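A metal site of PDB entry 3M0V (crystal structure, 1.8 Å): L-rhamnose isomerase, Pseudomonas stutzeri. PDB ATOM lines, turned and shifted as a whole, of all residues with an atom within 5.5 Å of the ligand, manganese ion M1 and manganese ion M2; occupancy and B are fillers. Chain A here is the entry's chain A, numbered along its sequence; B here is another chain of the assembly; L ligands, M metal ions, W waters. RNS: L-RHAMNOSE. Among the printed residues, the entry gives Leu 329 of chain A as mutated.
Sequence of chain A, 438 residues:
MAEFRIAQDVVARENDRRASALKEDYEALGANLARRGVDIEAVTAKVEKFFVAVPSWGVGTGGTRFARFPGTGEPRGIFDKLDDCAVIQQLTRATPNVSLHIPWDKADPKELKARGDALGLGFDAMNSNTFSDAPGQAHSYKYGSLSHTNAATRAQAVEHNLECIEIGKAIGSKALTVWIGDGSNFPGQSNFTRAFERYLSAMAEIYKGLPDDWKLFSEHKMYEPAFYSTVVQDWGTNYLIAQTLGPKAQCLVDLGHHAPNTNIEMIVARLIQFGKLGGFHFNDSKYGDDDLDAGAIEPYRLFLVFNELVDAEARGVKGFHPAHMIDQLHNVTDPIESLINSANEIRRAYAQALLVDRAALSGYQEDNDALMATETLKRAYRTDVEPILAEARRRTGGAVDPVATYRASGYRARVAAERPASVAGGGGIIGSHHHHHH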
ATOM      1  N   TRP A  57     -19.980  -3.899  24.763  1.00  0.00           N
ATOM      2  CA  TRP A  57     -20.356  -2.693  25.495  1.00  0.00           C
ATOM      3  C   TRP A  57     -20.933  -2.956  26.889  1.00  0.00           C
ATOM      4  O   TRP A  57     -21.228  -2.016  27.633  1.00  0.00           O
ATOM      5  CB  TRP A  57     -21.321  -1.856  24.657  1.00  0.00           C
ATOM      6  CG  TRP A  57     -22.622  -2.525  24.334  1.00  0.00           C
ATOM      7  CD1 TRP A  57     -23.782  -2.427  25.048  1.00  0.00           C
ATOM      8  CD2 TRP A  57     -22.897  -3.380  23.220  1.00  0.00           C
ATOM      9  NE1 TRP A  57     -24.774  -3.163  24.437  1.00  0.00           N
ATOM     10  CE2 TRP A  57     -24.258  -3.758  23.311  1.00  0.00           C
ATOM     11  CE3 TRP A  57     -22.133  -3.853  22.145  1.00  0.00           C
ATOM     12  CZ2 TRP A  57     -24.868  -4.594  22.368  1.00  0.00           C
ATOM     13  CZ3 TRP A  57     -22.746  -4.691  21.211  1.00  0.00           C
ATOM     14  CH2 TRP A  57     -24.092  -5.053  21.332  1.00  0.00           C
ATOM     15  N   HIS A 101     -19.135  -3.412  18.522  1.00  0.00           N
ATOM     16  CA  HIS A 101     -19.862  -2.185  18.227  1.00  0.00           C
ATOM     17  C   HIS A 101     -18.864  -1.190  17.632  1.00  0.00           C
ATOM     18  O   HIS A 101     -17.822  -0.910  18.227  1.00  0.00           O
ATOM     19  CB  HIS A 101     -20.487  -1.626  19.502  1.00  0.00           C
ATOM     20  CG  HIS A 101     -21.822  -0.984  19.300  1.00  0.00           C
ATOM     21  ND1 HIS A 101     -21.999   0.136  18.518  1.00  0.00           N
ATOM     22  CD2 HIS A 101     -23.047  -1.308  19.767  1.00  0.00           C
ATOM     23  CE1 HIS A 101     -23.276   0.479  18.530  1.00  0.00           C
ATOM     24  NE2 HIS A 101     -23.935  -0.386  19.277  1.00  0.00           N
ATOM     25  N   TRP A 104     -16.959   2.200  18.630  1.00  0.00           N
ATOM     26  CA  TRP A 104     -16.403   1.935  19.958  1.00  0.00           C
ATOM     27  C   TRP A 104     -15.277   0.918  19.933  1.00  0.00           C
ATOM     28  O   TRP A 104     -14.224   1.127  20.540  1.00  0.00           O
ATOM     29  CB  TRP A 104     -17.479   1.457  20.939  1.00  0.00           C
ATOM     30  CG  TRP A 104     -18.573   2.450  21.222  1.00  0.00           C
ATOM     31  CD1 TRP A 104     -18.502   3.812  21.099  1.00  0.00           C
ATOM     32  CD2 TRP A 104     -19.897   2.159  21.680  1.00  0.00           C
ATOM     33  NE1 TRP A 104     -19.706   4.386  21.465  1.00  0.00           N
ATOM     34  CE2 TRP A 104     -20.574   3.389  21.827  1.00  0.00           C
ATOM     35  CE3 TRP A 104     -20.572   0.969  21.989  1.00  0.00           C
ATOM     36  CZ2 TRP A 104     -21.908   3.465  22.255  1.00  0.00           C
ATOM     37  CZ3 TRP A 104     -21.893   1.049  22.422  1.00  0.00           C
ATOM     38  CH2 TRP A 104     -22.540   2.281  22.550  1.00  0.00           C
ATOM     39  N   ASN A 127     -22.426  -4.360  15.113  1.00  0.00           N
ATOM     40  CA  ASN A 127     -23.417  -3.345  15.471  1.00  0.00           C
ATOM     41  C   ASN A 127     -22.909  -2.003  15.009  1.00  0.00           C
ATOM     42  O   ASN A 127     -21.793  -1.613  15.349  1.00  0.00           O
ATOM     43  CB  ASN A 127     -23.621  -3.305  16.986  1.00  0.00           C
ATOM     44  CG  ASN A 127     -24.237  -4.580  17.518  1.00  0.00           C
ATOM     45  OD1 ASN A 127     -25.462  -4.714  17.599  1.00  0.00           O
ATOM     46  ND2 ASN A 127     -23.399  -5.528  17.898  1.00  0.00           N
ATOM     47  N   SER A 128     -23.717  -1.297  14.225  1.00  0.00           N
ATOM     48  CA  SER A 128     -23.356   0.031  13.727  1.00  0.00           C
ATOM     49  C   SER A 128     -23.784   1.079  14.746  1.00  0.00           C
ATOM     50  O   SER A 128     -24.643   0.827  15.592  1.00  0.00           O
ATOM     51  CB  SER A 128     -24.044   0.298  12.394  1.00  0.00           C
ATOM     52  OG  SER A 128     -25.459   0.183  12.504  1.00  0.00           O
ATOM     53  N   PHE A 131     -26.199   6.751  16.254  1.00  0.00           N
ATOM     54  CA  PHE A 131     -27.067   7.356  17.261  1.00  0.00           C
ATOM     55  C   PHE A 131     -26.228   8.292  18.125  1.00  0.00           C
ATOM     56  O   PHE A 131     -26.667   8.799  19.154  1.00  0.00           O
ATOM     57  CB  PHE A 131     -27.756   6.281  18.119  1.00  0.00           C
ATOM     58  CG  PHE A 131     -26.813   5.261  18.719  1.00  0.00           C
ATOM     59  CD1 PHE A 131     -26.043   5.566  19.836  1.00  0.00           C
ATOM     60  CD2 PHE A 131     -26.704   3.989  18.156  1.00  0.00           C
ATOM     61  CE1 PHE A 131     -25.187   4.622  20.397  1.00  0.00           C
ATOM     62  CE2 PHE A 131     -25.850   3.038  18.704  1.00  0.00           C
ATOM     63  CZ  PHE A 131     -25.083   3.357  19.822  1.00  0.00           C
ATOM     64  N   TRP A 179     -29.535  -0.577  14.892  1.00  0.00           N
ATOM     65  CA  TRP A 179     -30.449   0.082  15.828  1.00  0.00           C
ATOM     66  C   TRP A 179     -30.074   1.553  15.743  1.00  0.00           C
ATOM     67  O   TRP A 179     -28.911   1.912  15.910  1.00  0.00           O
ATOM     68  CB  TRP A 179     -30.261  -0.368  17.276  1.00  0.00           C
ATOM     69  CG  TRP A 179     -31.135   0.474  18.186  1.00  0.00           C
ATOM     70  CD1 TRP A 179     -32.490   0.437  18.258  1.00  0.00           C
ATOM     71  CD2 TRP A 179     -30.717   1.571  19.010  1.00  0.00           C
ATOM     72  NE1 TRP A 179     -32.955   1.443  19.071  1.00  0.00           N
ATOM     73  CE2 TRP A 179     -31.892   2.159  19.542  1.00  0.00           C
ATOM     74  CE3 TRP A 179     -29.471   2.121  19.343  1.00  0.00           C
ATOM     75  CZ2 TRP A 179     -31.848   3.270  20.391  1.00  0.00           C
ATOM     76  CZ3 TRP A 179     -29.435   3.222  20.199  1.00  0.00           C
ATOM     77  CH2 TRP A 179     -30.620   3.787  20.711  1.00  0.00           C
ATOM     78  N   GLU A 219     -33.558  -3.555  14.527  1.00  0.00           N
ATOM     79  CA  GLU A 219     -34.067  -3.643  15.904  1.00  0.00           C
ATOM     80  C   GLU A 219     -35.059  -2.525  16.248  1.00  0.00           C
ATOM     81  O   GLU A 219     -34.701  -1.346  16.252  1.00  0.00           O
ATOM     82  CB  GLU A 219     -32.876  -3.630  16.872  1.00  0.00           C
ATOM     83  CG  GLU A 219     -33.242  -3.571  18.352  1.00  0.00           C
ATOM     84  CD  GLU A 219     -32.021  -3.594  19.249  1.00  0.00           C
ATOM     85  OE1 GLU A 219     -30.917  -3.300  18.753  1.00  0.00           O
ATOM     86  OE2 GLU A 219     -32.165  -3.877  20.464  1.00  0.00           O
ATOM     87  N   LYS A 221     -37.716  -0.311  18.646  1.00  0.00           N
ATOM     88  CA  LYS A 221     -37.717   0.211  20.005  1.00  0.00           C
ATOM     89  C   LYS A 221     -38.815   1.264  20.113  1.00  0.00           C
ATOM     90  O   LYS A 221     -38.878   2.196  19.315  1.00  0.00           O
ATOM     91  CB  LYS A 221     -36.363   0.835  20.339  1.00  0.00           C
ATOM     92  CG  LYS A 221     -36.180   1.102  21.814  1.00  0.00           C
ATOM     93  CD  LYS A 221     -34.861   1.787  22.103  1.00  0.00           C
ATOM     94  CE  LYS A 221     -34.596   1.831  23.600  1.00  0.00           C
ATOM     95  NZ  LYS A 221     -33.329   2.568  23.890  1.00  0.00           N
ATOM     96  N   GLU A 224     -36.901   6.295  23.287  1.00  0.00           N
ATOM     97  CA  GLU A 224     -35.562   6.559  23.817  1.00  0.00           C
ATOM     98  C   GLU A 224     -34.505   6.160  22.789  1.00  0.00           C
ATOM     99  O   GLU A 224     -34.354   4.979  22.487  1.00  0.00           O
ATOM    100  CB  GLU A 224     -35.287   5.813  25.131  1.00  0.00           C
ATOM    101  CG  GLU A 224     -33.919   6.204  25.729  1.00  0.00           C
ATOM    102  CD  GLU A 224     -33.416   5.221  26.779  1.00  0.00           C
ATOM    103  OE1 GLU A 224     -33.659   4.005  26.648  1.00  0.00           O
ATOM    104  OE2 GLU A 224     -32.737   5.679  27.729  1.00  0.00           O
ATOM    105  N   LEU A 252     -34.848  -8.150  14.773  1.00  0.00           N
ATOM    106  CA  LEU A 252     -34.220  -8.479  16.040  1.00  0.00           C
ATOM    107  C   LEU A 252     -35.128  -7.967  17.156  1.00  0.00           C
ATOM    108  O   LEU A 252     -35.587  -6.824  17.129  1.00  0.00           O
ATOM    109  CB  LEU A 252     -32.834  -7.839  16.139  1.00  0.00           C
ATOM    110  CG  LEU A 252     -32.042  -8.261  17.384  1.00  0.00           C
ATOM    111  CD1 LEU A 252     -30.574  -8.440  17.030  1.00  0.00           C
ATOM    112  CD2 LEU A 252     -32.218  -7.226  18.484  1.00  0.00           C
ATOM    113  N   ASP A 254     -35.490  -7.101  21.061  1.00  0.00           N
ATOM    114  CA  ASP A 254     -34.796  -6.806  22.310  1.00  0.00           C
ATOM    115  C   ASP A 254     -35.922  -6.795  23.346  1.00  0.00           C
ATOM    116  O   ASP A 254     -36.840  -5.992  23.256  1.00  0.00           O
ATOM    117  CB  ASP A 254     -34.143  -5.424  22.247  1.00  0.00           C
ATOM    118  CG  ASP A 254     -33.346  -5.102  23.496  1.00  0.00           C
ATOM    119  OD1 ASP A 254     -33.917  -5.241  24.601  1.00  0.00           O
ATOM    120  OD2 ASP A 254     -32.162  -4.710  23.374  1.00  0.00           O
ATOM    121  N   HIS A 257     -37.671  -3.489  24.785  1.00  0.00           N
ATOM    122  CA  HIS A 257     -38.087  -2.442  23.845  1.00  0.00           C
ATOM    123  C   HIS A 257     -39.574  -2.394  23.494  1.00  0.00           C
ATOM    124  O   HIS A 257     -39.941  -1.881  22.436  1.00  0.00           O
ATOM    125  CB  HIS A 257     -37.300  -2.593  22.537  1.00  0.00           C
ATOM    126  CG  HIS A 257     -35.838  -2.296  22.663  1.00  0.00           C
ATOM    127  ND1 HIS A 257     -35.013  -2.192  21.570  1.00  0.00           N
ATOM    128  CD2 HIS A 257     -35.059  -2.082  23.755  1.00  0.00           C
ATOM    129  CE1 HIS A 257     -33.780  -1.917  21.975  1.00  0.00           C
ATOM    130  NE2 HIS A 257     -33.782  -1.847  23.290  1.00  0.00           N
ATOM    131  N   HIS A 281     -32.112  -9.927  21.701  1.00  0.00           N
ATOM    132  CA  HIS A 281     -31.228  -9.140  22.541  1.00  0.00           C
ATOM    133  C   HIS A 281     -31.853  -9.412  23.904  1.00  0.00           C
ATOM    134  O   HIS A 281     -32.923  -8.878  24.215  1.00  0.00           O
ATOM    135  CB  HIS A 281     -31.276  -7.644  22.216  1.00  0.00           C
ATOM    136  CG  HIS A 281     -30.176  -7.180  21.295  1.00  0.00           C
ATOM    137  ND1 HIS A 281     -29.909  -5.858  21.065  1.00  0.00           N
ATOM    138  CD2 HIS A 281     -29.303  -7.888  20.541  1.00  0.00           C
ATOM    139  CE1 HIS A 281     -28.919  -5.752  20.197  1.00  0.00           C
ATOM    140  NE2 HIS A 281     -28.534  -6.978  19.865  1.00  0.00           N
ATOM    141  N   ASN A 283     -32.250  -9.464  28.009  1.00  0.00           N
ATOM    142  CA  ASN A 283     -32.069  -8.602  29.176  1.00  0.00           C
ATOM    143  C   ASN A 283     -33.399  -8.642  29.920  1.00  0.00           C
ATOM    144  O   ASN A 283     -34.349  -9.261  29.445  1.00  0.00           O
ATOM    145  CB  ASN A 283     -31.730  -7.157  28.780  1.00  0.00           C
ATOM    146  CG  ASN A 283     -32.704  -6.576  27.747  1.00  0.00           C
ATOM    147  OD1 ASN A 283     -33.912  -6.470  27.989  1.00  0.00           O
ATOM    148  ND2 ASN A 283     -32.170  -6.172  26.604  1.00  0.00           N
ATOM    149  N   ASP A 289     -36.588   0.457  29.066  1.00  0.00           N
ATOM    150  CA  ASP A 289     -35.510  -0.362  28.519  1.00  0.00           C
ATOM    151  C   ASP A 289     -34.407  -0.373  29.580  1.00  0.00           C
ATOM    152  O   ASP A 289     -33.339   0.191  29.394  1.00  0.00           O
ATOM    153  CB  ASP A 289     -34.997   0.229  27.208  1.00  0.00           C
ATOM    154  CG  ASP A 289     -33.926  -0.621  26.565  1.00  0.00           C
ATOM    155  OD1 ASP A 289     -33.956  -1.853  26.761  1.00  0.00           O
ATOM    156  OD2 ASP A 289     -33.057  -0.055  25.860  1.00  0.00           O
ATOM    157  N   ASP A 291     -32.411  -2.677  30.683  1.00  0.00           N
ATOM    158  CA  ASP A 291     -31.188  -3.415  30.400  1.00  0.00           C
ATOM    159  C   ASP A 291     -30.599  -4.152  31.595  1.00  0.00           C
ATOM    160  O   ASP A 291     -29.384  -4.205  31.757  1.00  0.00           O
ATOM    161  CB  ASP A 291     -30.138  -2.472  29.803  1.00  0.00           C
ATOM    162  CG  ASP A 291     -30.431  -2.124  28.362  1.00  0.00           C
ATOM    163  OD1 ASP A 291     -30.798  -3.053  27.622  1.00  0.00           O
ATOM    164  OD2 ASP A 291     -30.313  -0.940  27.984  1.00  0.00           O
ATOM    165  N   ASP A 327     -27.927  -8.132  25.575  1.00  0.00           N
ATOM    166  CA  ASP A 327     -27.733  -6.699  25.437  1.00  0.00           C
ATOM    167  C   ASP A 327     -28.118  -6.118  26.783  1.00  0.00           C
ATOM    168  O   ASP A 327     -29.296  -5.844  27.047  1.00  0.00           O
ATOM    169  CB  ASP A 327     -28.595  -6.082  24.344  1.00  0.00           C
ATOM    170  CG  ASP A 327     -28.344  -4.587  24.185  1.00  0.00           C
ATOM    171  OD1 ASP A 327     -27.391  -4.086  24.833  1.00  0.00           O
ATOM    172  OD2 ASP A 327     -29.072  -3.914  23.435  1.00  0.00           O
ATOM    173  N   LEU A 329     -26.668  -3.614  30.391  1.00  0.00           N
ATOM    174  CA  LEU A 329     -25.783  -2.594  30.951  1.00  0.00           C
ATOM    175  C   LEU A 329     -25.728  -2.899  32.431  1.00  0.00           C
ATOM    176  O   LEU A 329     -26.748  -3.182  33.059  1.00  0.00           O
ATOM    177  CB  LEU A 329     -26.350  -1.189  30.718  1.00  0.00           C
ATOM    178  CG  LEU A 329     -26.198  -0.613  29.302  1.00  0.00           C
ATOM    179  CD1 LEU A 329     -24.721  -0.624  28.908  1.00  0.00           C
ATOM    180  CD2 LEU A 329     -27.003  -1.432  28.311  1.00  0.00           C
ATOM    181  N   ARG B  65     -28.771   8.904  27.642  1.00  0.00           N
ATOM    182  CA  ARG B  65     -27.624   8.053  27.961  1.00  0.00           C
ATOM    183  C   ARG B  65     -26.864   7.633  26.699  1.00  0.00           C
ATOM    184  O   ARG B  65     -25.722   7.177  26.788  1.00  0.00           O
ATOM    185  CB  ARG B  65     -28.060   6.818  28.752  1.00  0.00           C
ATOM    186  CG  ARG B  65     -29.111   5.957  28.052  1.00  0.00           C
ATOM    187  CD  ARG B  65     -29.347   4.633  28.793  1.00  0.00           C
ATOM    188  NE  ARG B  65     -30.486   3.918  28.240  1.00  0.00           N
ATOM    189  CZ  ARG B  65     -30.608   2.592  28.220  1.00  0.00           C
ATOM    190  NH1 ARG B  65     -29.670   1.814  28.735  1.00  0.00           N
ATOM    191  NH2 ARG B  65     -31.693   2.045  27.688  1.00  0.00           N
ATOM    192  N   PHE B  66     -27.492   7.797  25.541  1.00  0.00           N
ATOM    193  CA  PHE B  66     -26.880   7.410  24.274  1.00  0.00           C
ATOM    194  C   PHE B  66     -26.015   8.499  23.625  1.00  0.00           C
ATOM    195  O   PHE B  66     -25.028   8.188  22.957  1.00  0.00           O
ATOM    196  CB  PHE B  66     -27.960   6.989  23.268  1.00  0.00           C
ATOM    197  CG  PHE B  66     -28.668   5.723  23.660  1.00  0.00           C
ATOM    198  CD1 PHE B  66     -28.020   4.497  23.545  1.00  0.00           C
ATOM    199  CD2 PHE B  66     -29.959   5.767  24.173  1.00  0.00           C
ATOM    200  CE1 PHE B  66     -28.652   3.333  23.941  1.00  0.00           C
ATOM    201  CE2 PHE B  66     -30.602   4.606  24.576  1.00  0.00           C
ATOM    202  CZ  PHE B  66     -29.952   3.382  24.452  1.00  0.00           C
HETATM  203  C1  RNS L   1     -30.753   0.391  22.207  1.00  0.00           C
HETATM  204  C2  RNS L   1     -30.620  -1.033  21.689  1.00  0.00           C
HETATM  205  C3  RNS L   1     -29.276  -1.230  21.003  1.00  0.00           C
HETATM  206  C4  RNS L   1     -28.099  -0.769  21.868  1.00  0.00           C
HETATM  207  C5  RNS L   1     -26.770  -1.221  21.268  1.00  0.00           C
HETATM  208  C6  RNS L   1     -25.624  -0.748  22.146  1.00  0.00           C
HETATM  209  O1  RNS L   1     -31.636   0.658  23.025  1.00  0.00           O
HETATM  210  O2  RNS L   1     -30.757  -1.941  22.764  1.00  0.00           O
HETATM  211  O3  RNS L   1     -29.123  -2.607  20.674  1.00  0.00           O
HETATM  212  O4  RNS L   1     -28.225  -1.307  23.182  1.00  0.00           O
HETATM  213  O5  RNS L   1     -26.622  -0.686  19.962  1.00  0.00           O
HETATM  214 MN    MN M   1     -30.614  -4.037  21.978  1.00  0.00          MN
HETATM  215 MN    MN M   2     -32.080  -1.037  24.224  1.00  0.00          MN
HETATM  216  O   HOH W   1     -27.211  -2.415  17.987  1.00  0.00           O
HETATM  217  O   HOH W   2     -32.005  -2.498  25.456  1.00  0.00           O
HETATM  218  O   HOH W   3     -30.290  -0.520  25.166  1.00  0.00           O
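O1 of the ligand sits close to NZ of Lys 221, at 2.7 Å.
O5 of the ligand sits at hydrogen-bond distance from NE2 of His 101.
A ring nitrogen (ND1) of His 257 sits close to the side-chain carboxylate (OE2) of Glu 219, 3.5 Å away.
The side-chain carboxylate (OD1) of Asp 254 sits at hydrogen-bond distance from the side-chain amide nitrogen (ND2) of Asn 283.
O of Asp 327 lies within hydrogen-bond range of ND2 of Asn 283, at 2.9 Å.
The side-chain carboxylate (OD2) of Asp 289 sits close to the side-chain amino group (NZ) of Lys 221 (3.3 Å).
O of Asp 289 sits at hydrogen-bond distance from NH2 of Arg 65 of chain B.
OD1 of Asp 327 sits at hydrogen-bond distance from NE1 of Trp 57 (2.8 Å).
The side-chain amino group of Lys 221 lies within salt-bridge range of the side-chain carboxylate of Glu 224.
Residues that only touch the ligand: Trp 57 (3.4 Å), Trp 179 (3.4 Å) and Phe 66 of chain B (3.5 Å).
Hydrophobic or aromatic side chains within 4 Å of the ligand: Trp 57, His 101, Trp 179, His 257, His 281 and Phe 66 of chain B.
Along chain A the residues within 4 Å of the ligand span positions 57 to 327.
The nearest printed residue that does not touch the ligand is Phe 131 (4.01 Å).
Five residues have an atom within 4 Å of manganese ion M1: Glu 219, Asp 254, His 257, His 281 and Asp 327.
Residues that only touch manganese ion M2: Lys 221.
Within 4 Å of manganese ion M2: Lys 221, Asp 254, His 257 and Asp 289.
The nearest printed residue that does not touch manganese ion M2 is Asp 291 (4.2 Å).
Manganese ion M1 is bound by the side-chain carboxylate of Asp 327, a ring nitrogen (ND1) of His 281, the side-chain carboxylate of Glu 219, the side-chain carboxylate of Asp 254, an oxygen (O2) of the ligand and an oxygen (O3) of the ligand.
Manganese ion M1 has six donor atoms within binding distance.
Manganese ion M2 is bound by water W2, water W3, a ring nitrogen (NE2) of His 257, an oxygen (O1) of the ligand, the side-chain carboxylate (OD2) of Asp 289 and an oxygen (O2) of the ligand.
Manganese ion M2 has six donor atoms within binding distance.
Water W3 lies within hydrogen-bond range of OD2 of Asp 291 (2.8 Å) and O4 of the ligand (3.0 Å).
Water W1 bridges an oxygen (O5) of the ligand (2.7 Å) and the side-chain amide oxygen (OD1) of Asn 127 (2.9 Å).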
